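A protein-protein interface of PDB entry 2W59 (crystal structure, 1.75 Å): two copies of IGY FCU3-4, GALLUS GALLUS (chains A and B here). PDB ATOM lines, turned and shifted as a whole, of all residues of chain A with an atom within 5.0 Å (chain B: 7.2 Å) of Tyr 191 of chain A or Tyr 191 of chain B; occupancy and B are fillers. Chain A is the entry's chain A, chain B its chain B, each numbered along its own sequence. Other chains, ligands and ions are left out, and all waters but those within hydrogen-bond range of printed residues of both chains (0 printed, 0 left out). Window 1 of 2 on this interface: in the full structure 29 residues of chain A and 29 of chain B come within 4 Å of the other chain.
The backbone carbonyl oxygen of Val 167 of chain B sits at hydrogen-bond distance from the backbone NH of Lys 193 of chain B (2.9 Å). OG of Ser 192 of chain B sits close to O of Val 167 of chain B, at 3.4 Å. The side-chain hydroxyl of Ser 139 of chain A sits at hydrogen-bond distance from the side-chain hydroxyl of Tyr 191 of chain A (2.9 Å). The backbone carbonyl oxygen (O) of Leu 141 of chain B lies within hydrogen-bond range of the backbone NH (N) of Tyr 122 of chain B (2.8 Å). The side-chain hydroxyl (OG1) of Thr 168 of chain A is in hydrogen-bond range of the side-chain hydroxyl (OG) of Ser 192 of chain A, at 2.8 Å. The backbone NH (N) of Lys 193 of chain A is in hydrogen-bond range of the backbone carbonyl oxygen (O) of Val 167 of chain A.
Among the printed residues, pairs that only touch across the chains: Thr 137 of chain A with Leu 141 of chain B (3.9 Å), Leu 141 of chain A with Thr 137 of chain B (3.9 Å), Leu 141 of chain A with Tyr 191 of chain B (3.5 Å), Val 167 of chain A with Leu 172 of chain B (3.96 Å), Val 167 of chain A with Phe 189 of chain B (3.4 Å), Thr 168 of chain A with Leu 172 of chain B (3.7 Å), Thr 169 of chain A with Thr 169 of chain B (3.7 Å), Thr 169 of chain A with Leu 172 of chain B (3.8 Å), Thr 169 of chain A with Phe 189 of chain B (3.7 Å), Phe 189 of chain A with Val 167 of chain B (3.5 Å), Phe 189 of chain A with Thr 169 of chain B (3.8 Å), Phe 189 of chain A with Lys 193 of chain B (3.7 Å), Tyr 191 of chain A with Leu 141 of chain B (3.7 Å), Tyr 191 of chain A with Tyr 191 of chain B (3.5 Å) and Lys 193 of chain A with Phe 189 of chain B (3.8 Å).
Tyr 191 of chain B touches two residues of chain A. Of the printed residues of chain B, Thr 137 of chain A touches Leu 141. Printed residues of chain A within 4 Å of Lys 193 of chain B: Phe 189 (3.7 Å). Of the printed residues of chain A, Leu 172 of chain B touches Val 167, Thr 168 and Thr 169. Of the printed residues of chain B, Thr 169 of chain A touches Thr 169 (3.7 Å), Leu 172 (3.8 Å) and Phe 189 (3.7 Å). Of the printed residues of chain B, Lys 193 of chain A touches Phe 189. Ala 170 of chain B touches none of the printed residues of chain A. The nearest residue of chain A that does not touch Tyr 191 of chain B is Phe 189 of chain A (4.2 Å). The nearest printed residue of chain B that does not touch Leu 141 of chain A is Lys 193 of chain B (4.1 Å).
Printed residues of chain B that touch a printed residue of chain A: Thr 137, Leu 141, Val 167, Thr 169, Leu 172, Phe 189, Tyr 191 and Lys 193. Hydrophobic or aromatic side chains of chain B within 4 Å of the printed part of chain A: Leu 141, Val 167, Leu 172, Phe 189 and Tyr 191. Of the 13 printed residues of chain A, 8 touch a printed residue of chain B. Hydrophobic or aromatic side chains of chain A that line the printed part of chain B: Leu 141, Val 167, Phe 189 and Tyr 191. Among the printed residues, 15 pairs touch across the chains. Among the printed residues, no Asp or Glu carboxylate lies within 4 Å of a Lys or Arg side-chain nitrogen of the other chain.
Thr 137 of chain A touches Leu 141 of chain B, and with the chains exchanged Leu 141 of chain A touches Thr 137 of chain B. Leu 141 of chain A touches Tyr 191 of chain B, and with the chains exchanged Tyr 191 of chain A touches Leu 141 of chain B. Thr 169 of chain B touches its own counterpart, Thr 169 of chain A. Phe 189 of chain A touches Lys 193 of chain B, and with the chains exchanged Lys 193 of chain A touches Phe 189 of chain B. Positions printed for both chains: 124, 137, 139, 140, 141, 167, 168, 169, 189, 190, 191, 192 and 193. Of the 15 pairs that touch across the chains among the printed residues, 12 have their exchanged pair printed and touching as well.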
ATOM      1  N   PHE A 124      15.346  -6.953 -25.411  1.00  0.00           N
ATOM      2  CA  PHE A 124      14.551  -5.878 -25.983  1.00  0.00           C
ATOM      3  C   PHE A 124      14.450  -6.077 -27.482  1.00  0.00           C
ATOM      4  O   PHE A 124      15.465  -6.175 -28.162  1.00  0.00           O
ATOM      5  CB  PHE A 124      15.215  -4.529 -25.735  1.00  0.00           C
ATOM      6  CG  PHE A 124      15.249  -4.128 -24.285  1.00  0.00           C
ATOM      7  CD1 PHE A 124      14.085  -3.747 -23.636  1.00  0.00           C
ATOM      8  CD2 PHE A 124      16.443  -4.123 -23.582  1.00  0.00           C
ATOM      9  CE1 PHE A 124      14.110  -3.375 -22.299  1.00  0.00           C
ATOM     10  CE2 PHE A 124      16.476  -3.746 -22.247  1.00  0.00           C
ATOM     11  CZ  PHE A 124      15.308  -3.378 -21.608  1.00  0.00           C
ATOM     12  N   THR A 137      18.010  -3.184 -34.286  1.00  0.00           N
ATOM     13  CA  THR A 137      18.881  -3.574 -33.195  1.00  0.00           C
ATOM     14  C   THR A 137      18.153  -4.477 -32.231  1.00  0.00           C
ATOM     15  O   THR A 137      17.099  -4.110 -31.714  1.00  0.00           O
ATOM     16  CB  THR A 137      19.307  -2.337 -32.394  1.00  0.00           C
ATOM     17  OG1 THR A 137      19.900  -1.385 -33.282  1.00  0.00           O
ATOM     18  CG2 THR A 137      20.296  -2.737 -31.318  1.00  0.00           C
ATOM     19  N   SER A 139      18.662  -6.265 -28.552  1.00  0.00           N
ATOM     20  CA  SER A 139      19.584  -6.047 -27.455  1.00  0.00           C
ATOM     21  C   SER A 139      19.141  -6.742 -26.194  1.00  0.00           C
ATOM     22  O   SER A 139      18.037  -7.268 -26.104  1.00  0.00           O
ATOM     23  CB  SER A 139      19.820  -4.553 -27.227  1.00  0.00           C
ATOM     24  OG  SER A 139      18.611  -3.856 -27.025  1.00  0.00           O
ATOM     25  N   CYS A 140      20.045  -6.757 -25.225  1.00  0.00           N
ATOM     26  CA  CYS A 140      19.857  -7.489 -24.001  1.00  0.00           C
ATOM     27  C   CYS A 140      20.499  -6.718 -22.848  1.00  0.00           C
ATOM     28  O   CYS A 140      21.683  -6.415 -22.928  1.00  0.00           O
ATOM     29  CB  CYS A 140      20.573  -8.825 -24.178  1.00  0.00           C
ATOM     30  SG  CYS A 140      20.131 -10.037 -23.000  1.00  0.00           S
ATOM     31  N   LEU A 141      19.736  -6.406 -21.805  1.00  0.00           N
ATOM     32  CA  LEU A 141      20.299  -5.861 -20.588  1.00  0.00           C
ATOM     33  C   LEU A 141      20.466  -7.042 -19.649  1.00  0.00           C
ATOM     34  O   LEU A 141      19.527  -7.821 -19.444  1.00  0.00           O
ATOM     35  CB  LEU A 141      19.352  -4.837 -19.962  1.00  0.00           C
ATOM     36  CG  LEU A 141      19.644  -4.458 -18.510  1.00  0.00           C
ATOM     37  CD1 LEU A 141      21.033  -3.821 -18.366  1.00  0.00           C
ATOM     38  CD2 LEU A 141      18.561  -3.524 -17.978  1.00  0.00           C
ATOM     39  N   VAL A 167      28.084  -6.392 -30.111  1.00  0.00           N
ATOM     40  CA  VAL A 167      28.984  -5.686 -29.198  1.00  0.00           C
ATOM     41  C   VAL A 167      28.390  -5.699 -27.804  1.00  0.00           C
ATOM     42  O   VAL A 167      27.174  -5.609 -27.646  1.00  0.00           O
ATOM     43  CB  VAL A 167      29.253  -4.242 -29.679  1.00  0.00           C
ATOM     44  CG1 VAL A 167      27.948  -3.505 -29.880  1.00  0.00           C
ATOM     45  CG2 VAL A 167      30.197  -3.507 -28.714  1.00  0.00           C
ATOM     46  N   THR A 168      29.244  -5.863 -26.797  1.00  0.00           N
ATOM     47  CA  THR A 168      28.791  -5.903 -25.409  1.00  0.00           C
ATOM     48  C   THR A 168      29.582  -4.856 -24.641  1.00  0.00           C
ATOM     49  O   THR A 168      30.787  -4.740 -24.824  1.00  0.00           O
ATOM     50  CB  THR A 168      29.026  -7.290 -24.786  1.00  0.00           C
ATOM     51  OG1 THR A 168      28.283  -8.278 -25.522  1.00  0.00           O
ATOM     52  CG2 THR A 168      28.589  -7.311 -23.332  1.00  0.00           C
ATOM     53  N   THR A 169      28.902  -4.096 -23.792  1.00  0.00           N
ATOM     54  CA  THR A 169      29.560  -2.992 -23.094  1.00  0.00           C
ATOM     55  C   THR A 169      30.463  -3.519 -21.987  1.00  0.00           C
ATOM     56  O   THR A 169      30.250  -4.615 -21.459  1.00  0.00           O
ATOM     57  CB  THR A 169      28.530  -2.007 -22.511  1.00  0.00           C
ATOM     58  OG1 THR A 169      27.675  -2.691 -21.581  1.00  0.00           O
ATOM     59  CG2 THR A 169      27.680  -1.384 -23.635  1.00  0.00           C
ATOM     60  N   PHE A 189      26.299  -4.691 -14.302  1.00  0.00           N
ATOM     61  CA  PHE A 189      25.480  -4.900 -15.487  1.00  0.00           C
ATOM     62  C   PHE A 189      26.320  -4.788 -16.745  1.00  0.00           C
ATOM     63  O   PHE A 189      27.364  -4.136 -16.758  1.00  0.00           O
ATOM     64  CB  PHE A 189      24.323  -3.893 -15.553  1.00  0.00           C
ATOM     65  CG  PHE A 189      24.719  -2.542 -16.086  1.00  0.00           C
ATOM     66  CD1 PHE A 189      24.432  -2.192 -17.401  1.00  0.00           C
ATOM     67  CD2 PHE A 189      25.385  -1.631 -15.279  1.00  0.00           C
ATOM     68  CE1 PHE A 189      24.797  -0.952 -17.904  1.00  0.00           C
ATOM     69  CE2 PHE A 189      25.755  -0.390 -15.772  1.00  0.00           C
ATOM     70  CZ  PHE A 189      25.460  -0.048 -17.091  1.00  0.00           C
ATOM     71  N   VAL A 190      25.848  -5.439 -17.797  1.00  0.00           N
ATOM     72  CA  VAL A 190      26.354  -5.210 -19.139  1.00  0.00           C
ATOM     73  C   VAL A 190      25.159  -5.083 -20.060  1.00  0.00           C
ATOM     74  O   VAL A 190      24.059  -5.541 -19.738  1.00  0.00           O
ATOM     75  CB  VAL A 190      27.260  -6.351 -19.643  1.00  0.00           C
ATOM     76  CG1 VAL A 190      28.558  -6.414 -18.844  1.00  0.00           C
ATOM     77  CG2 VAL A 190      26.515  -7.710 -19.619  1.00  0.00           C
ATOM     78  N   TYR A 191      25.386  -4.463 -21.207  1.00  0.00           N
ATOM     79  CA  TYR A 191      24.369  -4.351 -22.233  1.00  0.00           C
ATOM     80  C   TYR A 191      24.984  -4.882 -23.524  1.00  0.00           C
ATOM     81  O   TYR A 191      26.133  -4.571 -23.837  1.00  0.00           O
ATOM     82  CB  TYR A 191      24.005  -2.880 -22.403  1.00  0.00           C
ATOM     83  CG  TYR A 191      23.098  -2.592 -23.569  1.00  0.00           C
ATOM     84  CD1 TYR A 191      23.606  -2.034 -24.731  1.00  0.00           C
ATOM     85  CD2 TYR A 191      21.740  -2.887 -23.516  1.00  0.00           C
ATOM     86  CE1 TYR A 191      22.788  -1.756 -25.811  1.00  0.00           C
ATOM     87  CE2 TYR A 191      20.909  -2.603 -24.601  1.00  0.00           C
ATOM     88  CZ  TYR A 191      21.449  -2.044 -25.741  1.00  0.00           C
ATOM     89  OH  TYR A 191      20.653  -1.747 -26.830  1.00  0.00           O
ATOM     90  N   SER A 192      24.244  -5.703 -24.257  1.00  0.00           N
ATOM     91  CA  SER A 192      24.753  -6.273 -25.498  1.00  0.00           C
ATOM     92  C   SER A 192      23.754  -6.010 -26.605  1.00  0.00           C
ATOM     93  O   SER A 192      22.541  -6.099 -26.392  1.00  0.00           O
ATOM     94  CB  SER A 192      24.996  -7.782 -25.340  1.00  0.00           C
ATOM     95  OG  SER A 192      25.688  -8.332 -26.456  1.00  0.00           O
ATOM     96  N   LYS A 193      24.250  -5.669 -27.792  1.00  0.00           N
ATOM     97  CA  LYS A 193      23.352  -5.418 -28.899  1.00  0.00           C
ATOM     98  C   LYS A 193      23.878  -6.050 -30.185  1.00  0.00           C
ATOM     99  O   LYS A 193      25.084  -6.237 -30.356  1.00  0.00           O
ATOM    100  CB  LYS A 193      23.120  -3.920 -29.081  1.00  0.00           C
ATOM    101  CG  LYS A 193      24.281  -3.187 -29.722  1.00  0.00           C
ATOM    102  CD  LYS A 193      23.876  -1.783 -30.158  1.00  0.00           C
ATOM    103  CE  LYS A 193      24.938  -1.137 -31.053  1.00  0.00           C
ATOM    104  NZ  LYS A 193      24.827  -1.470 -32.515  1.00  0.00           N
ATOM    105  N   TYR B 122      16.827   5.834 -28.807  1.00  0.00           N
ATOM    106  CA  TYR B 122      15.738   4.862 -28.655  1.00  0.00           C
ATOM    107  C   TYR B 122      15.470   4.529 -27.178  1.00  0.00           C
ATOM    108  O   TYR B 122      16.185   3.731 -26.586  1.00  0.00           O
ATOM    109  CB  TYR B 122      16.091   3.563 -29.386  1.00  0.00           C
ATOM    110  CG  TYR B 122      16.332   3.748 -30.867  1.00  0.00           C
ATOM    111  CD1 TYR B 122      15.284   4.063 -31.728  1.00  0.00           C
ATOM    112  CD2 TYR B 122      17.608   3.617 -31.403  1.00  0.00           C
ATOM    113  CE1 TYR B 122      15.508   4.226 -33.104  1.00  0.00           C
ATOM    114  CE2 TYR B 122      17.837   3.786 -32.772  1.00  0.00           C
ATOM    115  CZ  TYR B 122      16.782   4.092 -33.610  1.00  0.00           C
ATOM    116  OH  TYR B 122      17.033   4.264 -34.962  1.00  0.00           O
ATOM    117  N   PHE B 124      13.607   2.827 -23.977  1.00  0.00           N
ATOM    118  CA  PHE B 124      12.903   1.584 -23.701  1.00  0.00           C
ATOM    119  C   PHE B 124      12.188   1.621 -22.371  1.00  0.00           C
ATOM    120  O   PHE B 124      12.787   1.925 -21.340  1.00  0.00           O
ATOM    121  CB  PHE B 124      13.871   0.412 -23.718  1.00  0.00           C
ATOM    122  CG  PHE B 124      14.522   0.212 -25.049  1.00  0.00           C
ATOM    123  CD1 PHE B 124      13.881  -0.513 -26.037  1.00  0.00           C
ATOM    124  CD2 PHE B 124      15.748   0.776 -25.324  1.00  0.00           C
ATOM    125  CE1 PHE B 124      14.468  -0.691 -27.273  1.00  0.00           C
ATOM    126  CE2 PHE B 124      16.341   0.600 -26.558  1.00  0.00           C
ATOM    127  CZ  PHE B 124      15.699  -0.134 -27.527  1.00  0.00           C
ATOM    128  N   THR B 137      13.498  -0.636 -14.528  1.00  0.00           N
ATOM    129  CA  THR B 137      14.591   0.002 -15.252  1.00  0.00           C
ATOM    130  C   THR B 137      14.095   0.735 -16.482  1.00  0.00           C
ATOM    131  O   THR B 137      13.465   0.133 -17.348  1.00  0.00           O
ATOM    132  CB  THR B 137      15.601  -1.055 -15.751  1.00  0.00           C
ATOM    133  OG1 THR B 137      16.039  -1.855 -14.650  1.00  0.00           O
ATOM    134  CG2 THR B 137      16.802  -0.375 -16.417  1.00  0.00           C
ATOM    135  N   LEU B 138      14.363   2.037 -16.558  1.00  0.00           N
ATOM    136  CA  LEU B 138      14.150   2.780 -17.794  1.00  0.00           C
ATOM    137  C   LEU B 138      15.484   2.856 -18.490  1.00  0.00           C
ATOM    138  O   LEU B 138      16.512   2.978 -17.836  1.00  0.00           O
ATOM    139  CB  LEU B 138      13.674   4.206 -17.507  1.00  0.00           C
ATOM    140  CG  LEU B 138      12.392   4.346 -16.697  1.00  0.00           C
ATOM    141  CD1 LEU B 138      11.906   5.798 -16.736  1.00  0.00           C
ATOM    142  CD2 LEU B 138      11.337   3.407 -17.226  1.00  0.00           C
ATOM    143  N   SER B 139      15.500   2.761 -19.810  1.00  0.00           N
ATOM    144  CA  SER B 139      16.803   2.810 -20.458  1.00  0.00           C
ATOM    145  C   SER B 139      16.734   3.453 -21.818  1.00  0.00           C
ATOM    146  O   SER B 139      15.653   3.723 -22.343  1.00  0.00           O
ATOM    147  CB  SER B 139      17.468   1.431 -20.499  1.00  0.00           C
ATOM    148  OG  SER B 139      16.638   0.474 -21.115  1.00  0.00           O
ATOM    149  N   CYS B 140      17.909   3.736 -22.366  1.00  0.00           N
ATOM    150  CA  CYS B 140      18.018   4.483 -23.595  1.00  0.00           C
ATOM    151  C   CYS B 140      19.216   3.965 -24.385  1.00  0.00           C
ATOM    152  O   CYS B 140      20.320   3.946 -23.847  1.00  0.00           O
ATOM    153  CB  CYS B 140      18.246   5.947 -23.232  1.00  0.00           C
ATOM    154  SG  CYS B 140      17.925   7.066 -24.555  1.00  0.00           S
ATOM    155  N   LEU B 141      19.004   3.535 -25.630  1.00  0.00           N
ATOM    156  CA  LEU B 141      20.114   3.214 -26.518  1.00  0.00           C
ATOM    157  C   LEU B 141      20.322   4.436 -27.389  1.00  0.00           C
ATOM    158  O   LEU B 141      19.374   4.927 -28.004  1.00  0.00           O
ATOM    159  CB  LEU B 141      19.781   2.015 -27.421  1.00  0.00           C
ATOM    160  CG  LEU B 141      20.741   1.833 -28.604  1.00  0.00           C
ATOM    161  CD1 LEU B 141      22.162   1.556 -28.118  1.00  0.00           C
ATOM    162  CD2 LEU B 141      20.264   0.717 -29.542  1.00  0.00           C
ATOM    163  N   VAL B 142      21.553   4.933 -27.448  1.00  0.00           N
ATOM    164  CA  VAL B 142      21.861   6.043 -28.337  1.00  0.00           C
ATOM    165  C   VAL B 142      22.960   5.553 -29.279  1.00  0.00           C
ATOM    166  O   VAL B 142      24.007   5.104 -28.819  1.00  0.00           O
ATOM    167  CB  VAL B 142      22.347   7.248 -27.526  1.00  0.00           C
ATOM    168  CG1 VAL B 142      22.637   8.408 -28.452  1.00  0.00           C
ATOM    169  CG2 VAL B 142      21.286   7.621 -26.475  1.00  0.00           C
ATOM    170  N   ILE B 152      25.006  11.768 -21.782  1.00  0.00           N
ATOM    171  CA  ILE B 152      23.602  11.406 -21.611  1.00  0.00           C
ATOM    172  C   ILE B 152      23.137  11.945 -20.264  1.00  0.00           C
ATOM    173  O   ILE B 152      23.848  11.822 -19.263  1.00  0.00           O
ATOM    174  CB  ILE B 152      23.388   9.878 -21.610  1.00  0.00           C
ATOM    175  CG1 ILE B 152      23.935   9.230 -22.898  1.00  0.00           C
ATOM    176  CG2 ILE B 152      21.910   9.545 -21.425  1.00  0.00           C
ATOM    177  CD1 ILE B 152      23.381   9.839 -24.184  1.00  0.00           C
ATOM    178  N   TRP B 154      19.401  12.595 -17.728  1.00  0.00           N
ATOM    179  CA  TRP B 154      18.020  12.171 -17.566  1.00  0.00           C
ATOM    180  C   TRP B 154      17.193  13.257 -16.879  1.00  0.00           C
ATOM    181  O   TRP B 154      17.703  14.039 -16.069  1.00  0.00           O
ATOM    182  CB  TRP B 154      17.947  10.883 -16.742  1.00  0.00           C
ATOM    183  CG  TRP B 154      18.363   9.634 -17.460  1.00  0.00           C
ATOM    184  CD1 TRP B 154      19.640   9.163 -17.634  1.00  0.00           C
ATOM    185  CD2 TRP B 154      17.492   8.670 -18.065  1.00  0.00           C
ATOM    186  NE1 TRP B 154      19.611   7.967 -18.318  1.00  0.00           N
ATOM    187  CE2 TRP B 154      18.305   7.642 -18.591  1.00  0.00           C
ATOM    188  CE3 TRP B 154      16.103   8.574 -18.212  1.00  0.00           C
ATOM    189  CZ2 TRP B 154      17.777   6.540 -19.258  1.00  0.00           C
ATOM    190  CZ3 TRP B 154      15.578   7.479 -18.884  1.00  0.00           C
ATOM    191  CH2 TRP B 154      16.415   6.473 -19.392  1.00  0.00           C
ATOM    192  N   VAL B 167      23.218   5.326 -14.800  1.00  0.00           N
ATOM    193  CA  VAL B 167      24.536   4.908 -15.225  1.00  0.00           C
ATOM    194  C   VAL B 167      24.577   4.778 -16.738  1.00  0.00           C
ATOM    195  O   VAL B 167      23.630   4.291 -17.360  1.00  0.00           O
ATOM    196  CB  VAL B 167      24.972   3.598 -14.515  1.00  0.00           C
ATOM    197  CG1 VAL B 167      23.964   2.476 -14.757  1.00  0.00           C
ATOM    198  CG2 VAL B 167      26.386   3.207 -14.926  1.00  0.00           C
ATOM    199  N   THR B 168      25.677   5.240 -17.321  1.00  0.00           N
ATOM    200  CA  THR B 168      25.843   5.228 -18.774  1.00  0.00           C
ATOM    201  C   THR B 168      27.118   4.466 -19.132  1.00  0.00           C
ATOM    202  O   THR B 168      28.166   4.653 -18.501  1.00  0.00           O
ATOM    203  CB  THR B 168      25.917   6.669 -19.313  1.00  0.00           C
ATOM    204  OG1 THR B 168      24.727   7.382 -18.934  1.00  0.00           O
ATOM    205  CG2 THR B 168      26.049   6.673 -20.835  1.00  0.00           C
ATOM    206  N   THR B 169      27.030   3.598 -20.135  1.00  0.00           N
ATOM    207  CA  THR B 169      28.187   2.808 -20.549  1.00  0.00           C
ATOM    208  C   THR B 169      29.239   3.658 -21.273  1.00  0.00           C
ATOM    209  O   THR B 169      28.920   4.665 -21.907  1.00  0.00           O
ATOM    210  CB  THR B 169      27.763   1.613 -21.437  1.00  0.00           C
ATOM    211  OG1 THR B 169      27.179   2.104 -22.656  1.00  0.00           O
ATOM    212  CG2 THR B 169      26.739   0.750 -20.706  1.00  0.00           C
ATOM    213  N   ALA B 170      30.501   3.257 -21.153  1.00  0.00           N
ATOM    214  CA  ALA B 170      31.570   3.940 -21.878  1.00  0.00           C
ATOM    215  C   ALA B 170      31.356   3.740 -23.367  1.00  0.00           C
ATOM    216  O   ALA B 170      31.071   2.620 -23.814  1.00  0.00           O
ATOM    217  CB  ALA B 170      32.921   3.386 -21.477  1.00  0.00           C
ATOM    218  N   VAL B 171      31.524   4.818 -24.125  1.00  0.00           N
ATOM    219  CA  VAL B 171      31.270   4.792 -25.566  1.00  0.00           C
ATOM    220  C   VAL B 171      32.119   3.732 -26.276  1.00  0.00           C
ATOM    221  O   VAL B 171      33.302   3.547 -25.966  1.00  0.00           O
ATOM    222  CB  VAL B 171      31.478   6.202 -26.207  1.00  0.00           C
ATOM    223  CG1 VAL B 171      32.945   6.628 -26.160  1.00  0.00           C
ATOM    224  CG2 VAL B 171      30.961   6.214 -27.637  1.00  0.00           C
ATOM    225  N   LEU B 172      31.501   3.021 -27.216  1.00  0.00           N
ATOM    226  CA  LEU B 172      32.199   1.999 -27.992  1.00  0.00           C
ATOM    227  C   LEU B 172      31.839   2.122 -29.468  1.00  0.00           C
ATOM    228  O   LEU B 172      30.736   2.558 -29.806  1.00  0.00           O
ATOM    229  CB  LEU B 172      31.794   0.589 -27.521  1.00  0.00           C
ATOM    230  CG  LEU B 172      32.309   0.064 -26.173  1.00  0.00           C
ATOM    231  CD1 LEU B 172      31.617  -1.256 -25.781  1.00  0.00           C
ATOM    232  CD2 LEU B 172      33.812  -0.122 -26.226  1.00  0.00           C
ATOM    233  N   PHE B 189      28.133   4.001 -30.025  1.00  0.00           N
ATOM    234  CA  PHE B 189      26.906   3.904 -29.250  1.00  0.00           C
ATOM    235  C   PHE B 189      27.201   3.964 -27.761  1.00  0.00           C
ATOM    236  O   PHE B 189      28.312   3.654 -27.315  1.00  0.00           O
ATOM    237  CB  PHE B 189      26.144   2.595 -29.566  1.00  0.00           C
ATOM    238  CG  PHE B 189      26.681   1.383 -28.835  1.00  0.00           C
ATOM    239  CD1 PHE B 189      26.050   0.913 -27.683  1.00  0.00           C
ATOM    240  CD2 PHE B 189      27.814   0.730 -29.291  1.00  0.00           C
ATOM    241  CE1 PHE B 189      26.542  -0.202 -26.998  1.00  0.00           C
ATOM    242  CE2 PHE B 189      28.320  -0.383 -28.608  1.00  0.00           C
ATOM    243  CZ  PHE B 189      27.687  -0.838 -27.465  1.00  0.00           C
ATOM    244  N   VAL B 190      26.196   4.389 -26.999  1.00  0.00           N
ATOM    245  CA  VAL B 190      26.205   4.263 -25.549  1.00  0.00           C
ATOM    246  C   VAL B 190      24.837   3.778 -25.120  1.00  0.00           C
ATOM    247  O   VAL B 190      23.856   3.921 -25.856  1.00  0.00           O
ATOM    248  CB  VAL B 190      26.491   5.602 -24.820  1.00  0.00           C
ATOM    249  CG1 VAL B 190      27.940   6.036 -25.028  1.00  0.00           C
ATOM    250  CG2 VAL B 190      25.528   6.688 -25.268  1.00  0.00           C
ATOM    251  N   TYR B 191      24.772   3.214 -23.919  1.00  0.00           N
ATOM    252  CA  TYR B 191      23.504   2.776 -23.359  1.00  0.00           C
ATOM    253  C   TYR B 191      23.402   3.358 -21.964  1.00  0.00           C
ATOM    254  O   TYR B 191      24.382   3.366 -21.229  1.00  0.00           O
ATOM    255  CB  TYR B 191      23.495   1.255 -23.280  1.00  0.00           C
ATOM    256  CG  TYR B 191      22.328   0.668 -22.515  1.00  0.00           C
ATOM    257  CD1 TYR B 191      21.072   0.562 -23.096  1.00  0.00           C
ATOM    258  CD2 TYR B 191      22.501   0.188 -21.222  1.00  0.00           C
ATOM    259  CE1 TYR B 191      20.003   0.001 -22.394  1.00  0.00           C
ATOM    260  CE2 TYR B 191      21.446  -0.371 -20.519  1.00  0.00           C
ATOM    261  CZ  TYR B 191      20.205  -0.462 -21.113  1.00  0.00           C
ATOM    262  OH  TYR B 191      19.162  -1.019 -20.401  1.00  0.00           O
ATOM    263  N   SER B 192      22.231   3.874 -21.601  1.00  0.00           N
ATOM    264  CA  SER B 192      22.089   4.488 -20.278  1.00  0.00           C
ATOM    265  C   SER B 192      20.851   3.930 -19.616  1.00  0.00           C
ATOM    266  O   SER B 192      19.849   3.672 -20.277  1.00  0.00           O
ATOM    267  CB  SER B 192      21.979   6.013 -20.419  1.00  0.00           C
ATOM    268  OG  SER B 192      22.033   6.662 -19.155  1.00  0.00           O
ATOM    269  N   LYS B 193      20.909   3.707 -18.312  1.00  0.00           N
ATOM    270  CA  LYS B 193      19.734   3.175 -17.642  1.00  0.00           C
ATOM    271  C   LYS B 193      19.538   3.847 -16.301  1.00  0.00           C
ATOM    272  O   LYS B 193      20.486   4.335 -15.689  1.00  0.00           O
ATOM    273  CB  LYS B 193      19.823   1.654 -17.471  1.00  0.00           C
ATOM    274  CG  LYS B 193      20.778   1.213 -16.376  1.00  0.00           C
ATOM    275  CD  LYS B 193      20.860  -0.311 -16.271  1.00  0.00           C
ATOM    276  CE  LYS B 193      21.694  -0.736 -15.068  1.00  0.00           C
ATOM    277  NZ  LYS B 193      20.983  -0.528 -13.749  1.00  0.00           N
ATOM    278  N   MET B 194      18.292   3.865 -15.852  1.00  0.00           N
ATOM    279  CA  MET B 194      17.946   4.532 -14.608  1.00  0.00           C
ATOM    280  C   MET B 194      16.872   3.721 -13.915  1.00  0.00           C
ATOM    281  O   MET B 194      15.810   3.477 -14.482  1.00  0.00           O
ATOM    282  CB  MET B 194      17.419   5.940 -14.887  1.00  0.00           C
ATOM    283  CG  MET B 194      16.976   6.675 -13.632  1.00  0.00           C
ATOM    284  SD  MET B 194      16.472   8.373 -13.976  1.00  0.00           S
ATOM    285  CE  MET B 194      15.026   8.125 -14.997  1.00  0.00           C
